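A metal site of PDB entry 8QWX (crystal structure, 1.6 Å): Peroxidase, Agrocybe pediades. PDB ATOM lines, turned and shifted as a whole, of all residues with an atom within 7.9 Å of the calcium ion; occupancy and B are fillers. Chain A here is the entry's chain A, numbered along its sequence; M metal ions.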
ATOM      1  N   ASN A 116     -14.070  17.627  -8.046  1.00  0.00           N
ATOM      2  CA  ASN A 116     -13.955  17.812  -9.480  1.00  0.00           C
ATOM      3  C   ASN A 116     -13.014  18.973  -9.800  1.00  0.00           C
ATOM      4  O   ASN A 116     -13.275  20.118  -9.393  1.00  0.00           O
ATOM      5  CB  ASN A 116     -15.341  18.039 -10.051  1.00  0.00           C
ATOM      6  CG  ASN A 116     -15.374  18.064 -11.560  1.00  0.00           C
ATOM      7  OD1 ASN A 116     -14.967  19.029 -12.188  1.00  0.00           O
ATOM      8  ND2 ASN A 116     -15.965  17.022 -12.146  1.00  0.00           N
ATOM      9  N   GLY A 168      -7.376  31.634  -2.913  1.00  0.00           N
ATOM     10  CA  GLY A 168      -8.543  31.638  -3.774  1.00  0.00           C
ATOM     11  C   GLY A 168      -9.012  30.243  -4.184  1.00  0.00           C
ATOM     12  O   GLY A 168     -10.202  29.916  -4.122  1.00  0.00           O
ATOM     13  N   GLY A 169      -8.073  29.409  -4.649  1.00  0.00           N
ATOM     14  CA  GLY A 169      -8.373  28.042  -5.008  1.00  0.00           C
ATOM     15  C   GLY A 169      -9.040  27.260  -3.886  1.00  0.00           C
ATOM     16  O   GLY A 169     -10.046  26.614  -4.070  1.00  0.00           O
ATOM     17  N   SER A 170      -8.477  27.353  -2.661  1.00  0.00           N
ATOM     18  CA  SER A 170      -9.068  26.666  -1.533  1.00  0.00           C
ATOM     19  C   SER A 170     -10.502  27.152  -1.290  1.00  0.00           C
ATOM     20  O   SER A 170     -11.383  26.337  -0.963  1.00  0.00           O
ATOM     21  CB  SER A 170      -8.265  26.854  -0.297  1.00  0.00           C
ATOM     22  OG  SER A 170      -7.047  26.162  -0.442  1.00  0.00           O
ATOM     23  N   HIS A 171     -10.730  28.444  -1.464  1.00  0.00           N
ATOM     24  CA  HIS A 171     -12.037  29.036  -1.185  1.00  0.00           C
ATOM     25  C   HIS A 171     -13.033  28.682  -2.285  1.00  0.00           C
ATOM     26  O   HIS A 171     -14.233  28.966  -2.118  1.00  0.00           O
ATOM     27  CB  HIS A 171     -11.959  30.529  -0.850  1.00  0.00           C
ATOM     28  CG  HIS A 171     -11.329  30.729   0.515  1.00  0.00           C
ATOM     29  ND1 HIS A 171     -11.038  31.968   1.002  1.00  0.00           N
ATOM     30  CD2 HIS A 171     -10.810  29.841   1.408  1.00  0.00           C
ATOM     31  CE1 HIS A 171     -10.382  31.807   2.174  1.00  0.00           C
ATOM     32  NE2 HIS A 171     -10.326  30.557   2.471  1.00  0.00           N
ATOM     33  N   SER A 172     -12.557  28.085  -3.375  1.00  0.00           N
ATOM     34  CA  SER A 172     -13.467  27.560  -4.371  1.00  0.00           C
ATOM     35  C   SER A 172     -14.192  26.327  -3.846  1.00  0.00           C
ATOM     36  O   SER A 172     -15.210  25.945  -4.429  1.00  0.00           O
ATOM     37  CB  SER A 172     -12.752  27.220  -5.676  1.00  0.00           C
ATOM     38  OG  SER A 172     -13.683  26.813  -6.664  1.00  0.00           O
ATOM     39  N   VAL A 173     -13.664  25.641  -2.809  1.00  0.00           N
ATOM     40  CA  VAL A 173     -14.251  24.416  -2.261  1.00  0.00           C
ATOM     41  C   VAL A 173     -14.313  24.537  -0.745  1.00  0.00           C
ATOM     42  O   VAL A 173     -13.560  23.883  -0.015  1.00  0.00           O
ATOM     43  CB  VAL A 173     -13.400  23.194  -2.713  1.00  0.00           C
ATOM     44  CG1 VAL A 173     -13.695  22.880  -4.167  1.00  0.00           C
ATOM     45  CG2 VAL A 173     -11.920  23.383  -2.485  1.00  0.00           C
ATOM     46  N   ALA A 174     -15.172  25.452  -0.274  1.00  0.00           N
ATOM     47  CA  ALA A 174     -15.097  25.887   1.110  1.00  0.00           C
ATOM     48  C   ALA A 174     -16.368  26.608   1.514  1.00  0.00           C
ATOM     49  O   ALA A 174     -16.988  27.320   0.721  1.00  0.00           O
ATOM     50  CB  ALA A 174     -13.913  26.817   1.251  1.00  0.00           C
ATOM     51  N   PRO A 187     -21.248  28.854   1.660  1.00  0.00           N
ATOM     52  CA  PRO A 187     -20.118  28.763   0.740  1.00  0.00           C
ATOM     53  C   PRO A 187     -19.532  30.123   0.382  1.00  0.00           C
ATOM     54  O   PRO A 187     -20.229  31.124   0.377  1.00  0.00           O
ATOM     55  CB  PRO A 187     -20.607  28.028  -0.491  1.00  0.00           C
ATOM     56  CG  PRO A 187     -22.091  27.997  -0.273  1.00  0.00           C
ATOM     57  CD  PRO A 187     -22.528  28.424   1.068  1.00  0.00           C
ATOM     58  N   PHE A 188     -18.245  30.115   0.000  1.00  0.00           N
ATOM     59  CA  PHE A 188     -17.635  31.338  -0.521  1.00  0.00           C
ATOM     60  C   PHE A 188     -17.937  31.536  -2.004  1.00  0.00           C
ATOM     61  O   PHE A 188     -17.938  32.679  -2.484  1.00  0.00           O
ATOM     62  CB  PHE A 188     -16.110  31.255  -0.313  1.00  0.00           C
ATOM     63  CG  PHE A 188     -15.693  31.255   1.155  1.00  0.00           C
ATOM     64  CD1 PHE A 188     -16.100  32.224   2.048  1.00  0.00           C
ATOM     65  CD2 PHE A 188     -14.838  30.266   1.617  1.00  0.00           C
ATOM     66  CE1 PHE A 188     -15.740  32.171   3.387  1.00  0.00           C
ATOM     67  CE2 PHE A 188     -14.439  30.243   2.947  1.00  0.00           C
ATOM     68  CZ  PHE A 188     -14.885  31.189   3.820  1.00  0.00           C
ATOM     69  N   ASP A 189     -18.114  30.455  -2.754  1.00  0.00           N
ATOM     70  CA  ASP A 189     -18.457  30.556  -4.170  1.00  0.00           C
ATOM     71  C   ASP A 189     -19.719  29.742  -4.450  1.00  0.00           C
ATOM     72  O   ASP A 189     -20.282  29.109  -3.573  1.00  0.00           O
ATOM     73  CB  ASP A 189     -17.297  30.313  -5.127  1.00  0.00           C
ATOM     74  CG  ASP A 189     -16.974  28.885  -5.568  1.00  0.00           C
ATOM     75  OD1 ASP A 189     -17.622  27.922  -5.084  1.00  0.00           O
ATOM     76  OD2 ASP A 189     -16.011  28.756  -6.365  1.00  0.00           O
ATOM     77  N   GLN A 190     -20.183  29.844  -5.694  1.00  0.00           N
ATOM     78  CA  GLN A 190     -21.446  29.241  -6.107  1.00  0.00           C
ATOM     79  C   GLN A 190     -21.387  27.707  -6.135  1.00  0.00           C
ATOM     80  O   GLN A 190     -22.425  27.039  -6.252  1.00  0.00           O
ATOM     81  CB  GLN A 190     -21.790  29.725  -7.500  1.00  0.00           C
ATOM     82  CG  GLN A 190     -22.163  31.195  -7.593  1.00  0.00           C
ATOM     83  CD  GLN A 190     -21.994  31.702  -9.001  1.00  0.00           C
ATOM     84  OE1 GLN A 190     -20.921  32.147  -9.437  1.00  0.00           O
ATOM     85  NE2 GLN A 190     -23.020  31.460  -9.792  1.00  0.00           N
ATOM     86  N   THR A 191     -20.169  27.156  -6.100  1.00  0.00           N
ATOM     87  CA  THR A 191     -19.900  25.750  -6.364  1.00  0.00           C
ATOM     88  C   THR A 191     -18.888  25.190  -5.364  1.00  0.00           C
ATOM     89  O   THR A 191     -17.770  24.820  -5.744  1.00  0.00           O
ATOM     90  CB  THR A 191     -19.369  25.611  -7.800  1.00  0.00           C
ATOM     91  OG1 THR A 191     -18.200  26.427  -7.958  1.00  0.00           O
ATOM     92  CG2 THR A 191     -20.395  25.981  -8.850  1.00  0.00           C
ATOM     93  N   PRO A 192     -19.257  25.011  -4.073  1.00  0.00           N
ATOM     94  CA  PRO A 192     -18.283  24.545  -3.094  1.00  0.00           C
ATOM     95  C   PRO A 192     -17.848  23.101  -3.266  1.00  0.00           C
ATOM     96  O   PRO A 192     -16.885  22.724  -2.621  1.00  0.00           O
ATOM     97  CB  PRO A 192     -18.987  24.750  -1.766  1.00  0.00           C
ATOM     98  CG  PRO A 192     -20.442  24.583  -2.147  1.00  0.00           C
ATOM     99  CD  PRO A 192     -20.555  25.325  -3.465  1.00  0.00           C
ATOM    100  N   SER A 193     -18.521  22.313  -4.146  1.00  0.00           N
ATOM    101  CA  SER A 193     -18.075  20.952  -4.441  1.00  0.00           C
ATOM    102  C   SER A 193     -17.263  20.864  -5.736  1.00  0.00           C
ATOM    103  O   SER A 193     -16.863  19.756  -6.125  1.00  0.00           O
ATOM    104  CB  SER A 193     -19.252  19.987  -4.519  1.00  0.00           C
ATOM    105  OG  SER A 193     -19.998  20.129  -5.724  1.00  0.00           O
ATOM    106  N   ILE A 194     -16.966  22.001  -6.384  1.00  0.00           N
ATOM    107  CA  ILE A 194     -16.228  21.976  -7.639  1.00  0.00           C
ATOM    108  C   ILE A 194     -15.027  22.918  -7.522  1.00  0.00           C
ATOM    109  O   ILE A 194     -15.190  24.085  -7.198  1.00  0.00           O
ATOM    110  CB  ILE A 194     -17.130  22.410  -8.809  1.00  0.00           C
ATOM    111  CG1 ILE A 194     -18.351  21.509  -8.954  1.00  0.00           C
ATOM    112  CG2 ILE A 194     -16.355  22.423 -10.137  1.00  0.00           C
ATOM    113  CD1 ILE A 194     -19.410  22.085  -9.863  1.00  0.00           C
ATOM    114  N   PHE A 195     -13.848  22.409  -7.884  1.00  0.00           N
ATOM    115  CA  PHE A 195     -12.630  23.196  -7.867  1.00  0.00           C
ATOM    116  C   PHE A 195     -12.518  23.964  -9.179  1.00  0.00           C
ATOM    117  O   PHE A 195     -11.753  23.584 -10.042  1.00  0.00           O
ATOM    118  CB  PHE A 195     -11.464  22.247  -7.609  1.00  0.00           C
ATOM    119  CG  PHE A 195     -10.174  22.943  -7.233  1.00  0.00           C
ATOM    120  CD1 PHE A 195      -9.935  23.298  -5.896  1.00  0.00           C
ATOM    121  CD2 PHE A 195      -9.210  23.287  -8.169  1.00  0.00           C
ATOM    122  CE1 PHE A 195      -8.768  23.939  -5.539  1.00  0.00           C
ATOM    123  CE2 PHE A 195      -8.053  23.961  -7.800  1.00  0.00           C
ATOM    124  CZ  PHE A 195      -7.839  24.290  -6.484  1.00  0.00           C
ATOM    125  N   ASP A 196     -13.305  25.005  -9.264  1.00  0.00           N
ATOM    126  CA  ASP A 196     -13.419  25.853 -10.460  1.00  0.00           C
ATOM    127  C   ASP A 196     -12.973  27.259 -10.106  1.00  0.00           C
ATOM    128  O   ASP A 196     -12.460  27.524  -9.004  1.00  0.00           O
ATOM    129  CB  ASP A 196     -14.837  25.813 -11.000  1.00  0.00           C
ATOM    130  CG  ASP A 196     -15.904  26.242 -10.009  1.00  0.00           C
ATOM    131  OD1 ASP A 196     -15.495  26.767  -8.929  1.00  0.00           O
ATOM    132  OD2 ASP A 196     -17.112  26.061 -10.323  1.00  0.00           O
ATOM    133  N   THR A 197     -13.109  28.193 -11.068  1.00  0.00           N
ATOM    134  CA  THR A 197     -12.684  29.559 -10.829  1.00  0.00           C
ATOM    135  C   THR A 197     -13.859  30.482 -10.508  1.00  0.00           C
ATOM    136  O   THR A 197     -13.687  31.705 -10.527  1.00  0.00           O
ATOM    137  CB  THR A 197     -11.866  30.086 -12.015  1.00  0.00           C
ATOM    138  OG1 THR A 197     -12.708  30.286 -13.161  1.00  0.00           O
ATOM    139  CG2 THR A 197     -10.765  29.133 -12.382  1.00  0.00           C
ATOM    140  N   GLN A 198     -15.036  29.950 -10.094  1.00  0.00           N
ATOM    141  CA  GLN A 198     -16.160  30.789  -9.736  1.00  0.00           C
ATOM    142  C   GLN A 198     -15.823  31.739  -8.580  1.00  0.00           C
ATOM    143  O   GLN A 198     -16.317  32.855  -8.566  1.00  0.00           O
ATOM    144  CB  GLN A 198     -17.423  29.958  -9.472  1.00  0.00           C
ATOM    145  CG  GLN A 198     -18.112  29.390 -10.722  1.00  0.00           C
ATOM    146  CD  GLN A 198     -18.358  30.425 -11.803  1.00  0.00           C
ATOM    147  OE1 GLN A 198     -17.807  30.293 -12.899  1.00  0.00           O
ATOM    148  NE2 GLN A 198     -19.122  31.459 -11.548  1.00  0.00           N
ATOM    149  N   ILE A 199     -15.007  31.297  -7.624  1.00  0.00           N
ATOM    150  CA  ILE A 199     -14.599  32.125  -6.479  1.00  0.00           C
ATOM    151  C   ILE A 199     -13.967  33.432  -6.985  1.00  0.00           C
ATOM    152  O   ILE A 199     -14.250  34.527  -6.460  1.00  0.00           O
ATOM    153  CB  ILE A 199     -13.639  31.353  -5.568  1.00  0.00           C
ATOM    154  CG1 ILE A 199     -13.178  32.191  -4.359  1.00  0.00           C
ATOM    155  CG2 ILE A 199     -12.403  30.833  -6.305  1.00  0.00           C
ATOM    156  CD1 ILE A 199     -14.301  32.508  -3.416  1.00  0.00           C
ATOM    157  N   PHE A 200     -13.179  33.336  -8.059  1.00  0.00           N
ATOM    158  CA  PHE A 200     -12.488  34.503  -8.563  1.00  0.00           C
ATOM    159  C   PHE A 200     -13.493  35.491  -9.141  1.00  0.00           C
ATOM    160  O   PHE A 200     -13.341  36.692  -8.921  1.00  0.00           O
ATOM    161  CB  PHE A 200     -11.365  34.181  -9.569  1.00  0.00           C
ATOM    162  CG  PHE A 200     -10.242  33.362  -8.949  1.00  0.00           C
ATOM    163  CD1 PHE A 200      -9.255  34.002  -8.208  1.00  0.00           C
ATOM    164  CD2 PHE A 200     -10.253  31.971  -8.942  1.00  0.00           C
ATOM    165  CE1 PHE A 200      -8.238  33.290  -7.590  1.00  0.00           C
ATOM    166  CE2 PHE A 200      -9.241  31.258  -8.283  1.00  0.00           C
ATOM    167  CZ  PHE A 200      -8.257  31.927  -7.600  1.00  0.00           C
ATOM    168  N   ASP A 202     -16.821  35.550  -8.360  1.00  0.00           N
ATOM    169  CA  ASP A 202     -17.791  35.905  -7.337  1.00  0.00           C
ATOM    170  C   ASP A 202     -17.267  37.066  -6.485  1.00  0.00           C
ATOM    171  O   ASP A 202     -18.008  37.979  -6.110  1.00  0.00           O
ATOM    172  CB  ASP A 202     -18.170  34.718  -6.485  1.00  0.00           C
ATOM    173  CG  ASP A 202     -18.971  33.641  -7.217  1.00  0.00           C
ATOM    174  OD1 ASP A 202     -19.549  33.947  -8.291  1.00  0.00           O
ATOM    175  OD2 ASP A 202     -19.050  32.517  -6.702  1.00  0.00           O
ATOM    176  N   MET A 256      -4.864  27.650 -12.751  1.00  0.00           N
ATOM    177  CA  MET A 256      -5.107  27.828 -11.325  1.00  0.00           C
ATOM    178  C   MET A 256      -4.789  26.539 -10.556  1.00  0.00           C
ATOM    179  O   MET A 256      -4.028  26.555  -9.543  1.00  0.00           O
ATOM    180  CB  MET A 256      -6.553  28.291 -11.134  1.00  0.00           C
ATOM    181  CG  MET A 256      -6.833  28.751  -9.723  1.00  0.00           C
ATOM    182  SD  MET A 256      -7.260  27.370  -8.666  1.00  0.00           S
ATOM    183  CE  MET A 256      -8.952  27.257  -9.266  1.00  0.00           C
ATOM    184  N   PHE A 290     -11.525  18.019 -14.361  1.00  0.00           N
ATOM    185  CA  PHE A 290     -12.474  19.126 -14.416  1.00  0.00           C
ATOM    186  C   PHE A 290     -13.423  18.863 -15.577  1.00  0.00           C
ATOM    187  O   PHE A 290     -12.958  18.634 -16.707  1.00  0.00           O
ATOM    188  CB  PHE A 290     -11.720  20.440 -14.618  1.00  0.00           C
ATOM    189  CG  PHE A 290     -12.656  21.628 -14.541  1.00  0.00           C
ATOM    190  CD1 PHE A 290     -13.451  21.830 -13.415  1.00  0.00           C
ATOM    191  CD2 PHE A 290     -12.769  22.539 -15.593  1.00  0.00           C
ATOM    192  CE1 PHE A 290     -14.317  22.918 -13.361  1.00  0.00           C
ATOM    193  CE2 PHE A 290     -13.637  23.632 -15.509  1.00  0.00           C
ATOM    194  CZ  PHE A 290     -14.399  23.806 -14.415  1.00  0.00           C
HETATM  195 CA    CA M   1     -16.091  26.313  -6.596  1.00  0.00          CA
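The backbone NH of Ile 199 sits close to the side-chain carboxylate of Asp 189 (3.0 Å).
OD1 of Asp 196 lies close to N of Gln 198, 3.4 Å away.
Within 4 Å of the calcium ion: Ser 172, Asp 189, Thr 191, Ile 194 and Asp 196.
The nearest printed residue that does not touch the calcium ion is Pro 192 (4.3 Å).
The calcium ion is bound by the backbone carbonyl oxygen (O) of Ser 172 (2.4 Å).
O of Thr 191 binds the calcium ion, at 2.4 Å.
OD1 of Asp 196 binds the calcium ion.
OD2 of Asp 189 is bound to the calcium ion, 2.5 Å away.
OG of Ser 172 binds the calcium ion (2.5 Å).
O of Ile 194 is bound to the calcium ion, 2.5 Å away.
OG1 of Thr 191 is bound to the calcium ion (2.5 Å).
The side-chain carboxylate (OD1) of Asp 189 binds the calcium ion (2.7 Å).
The calcium ion has eight donor atoms within binding distance.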
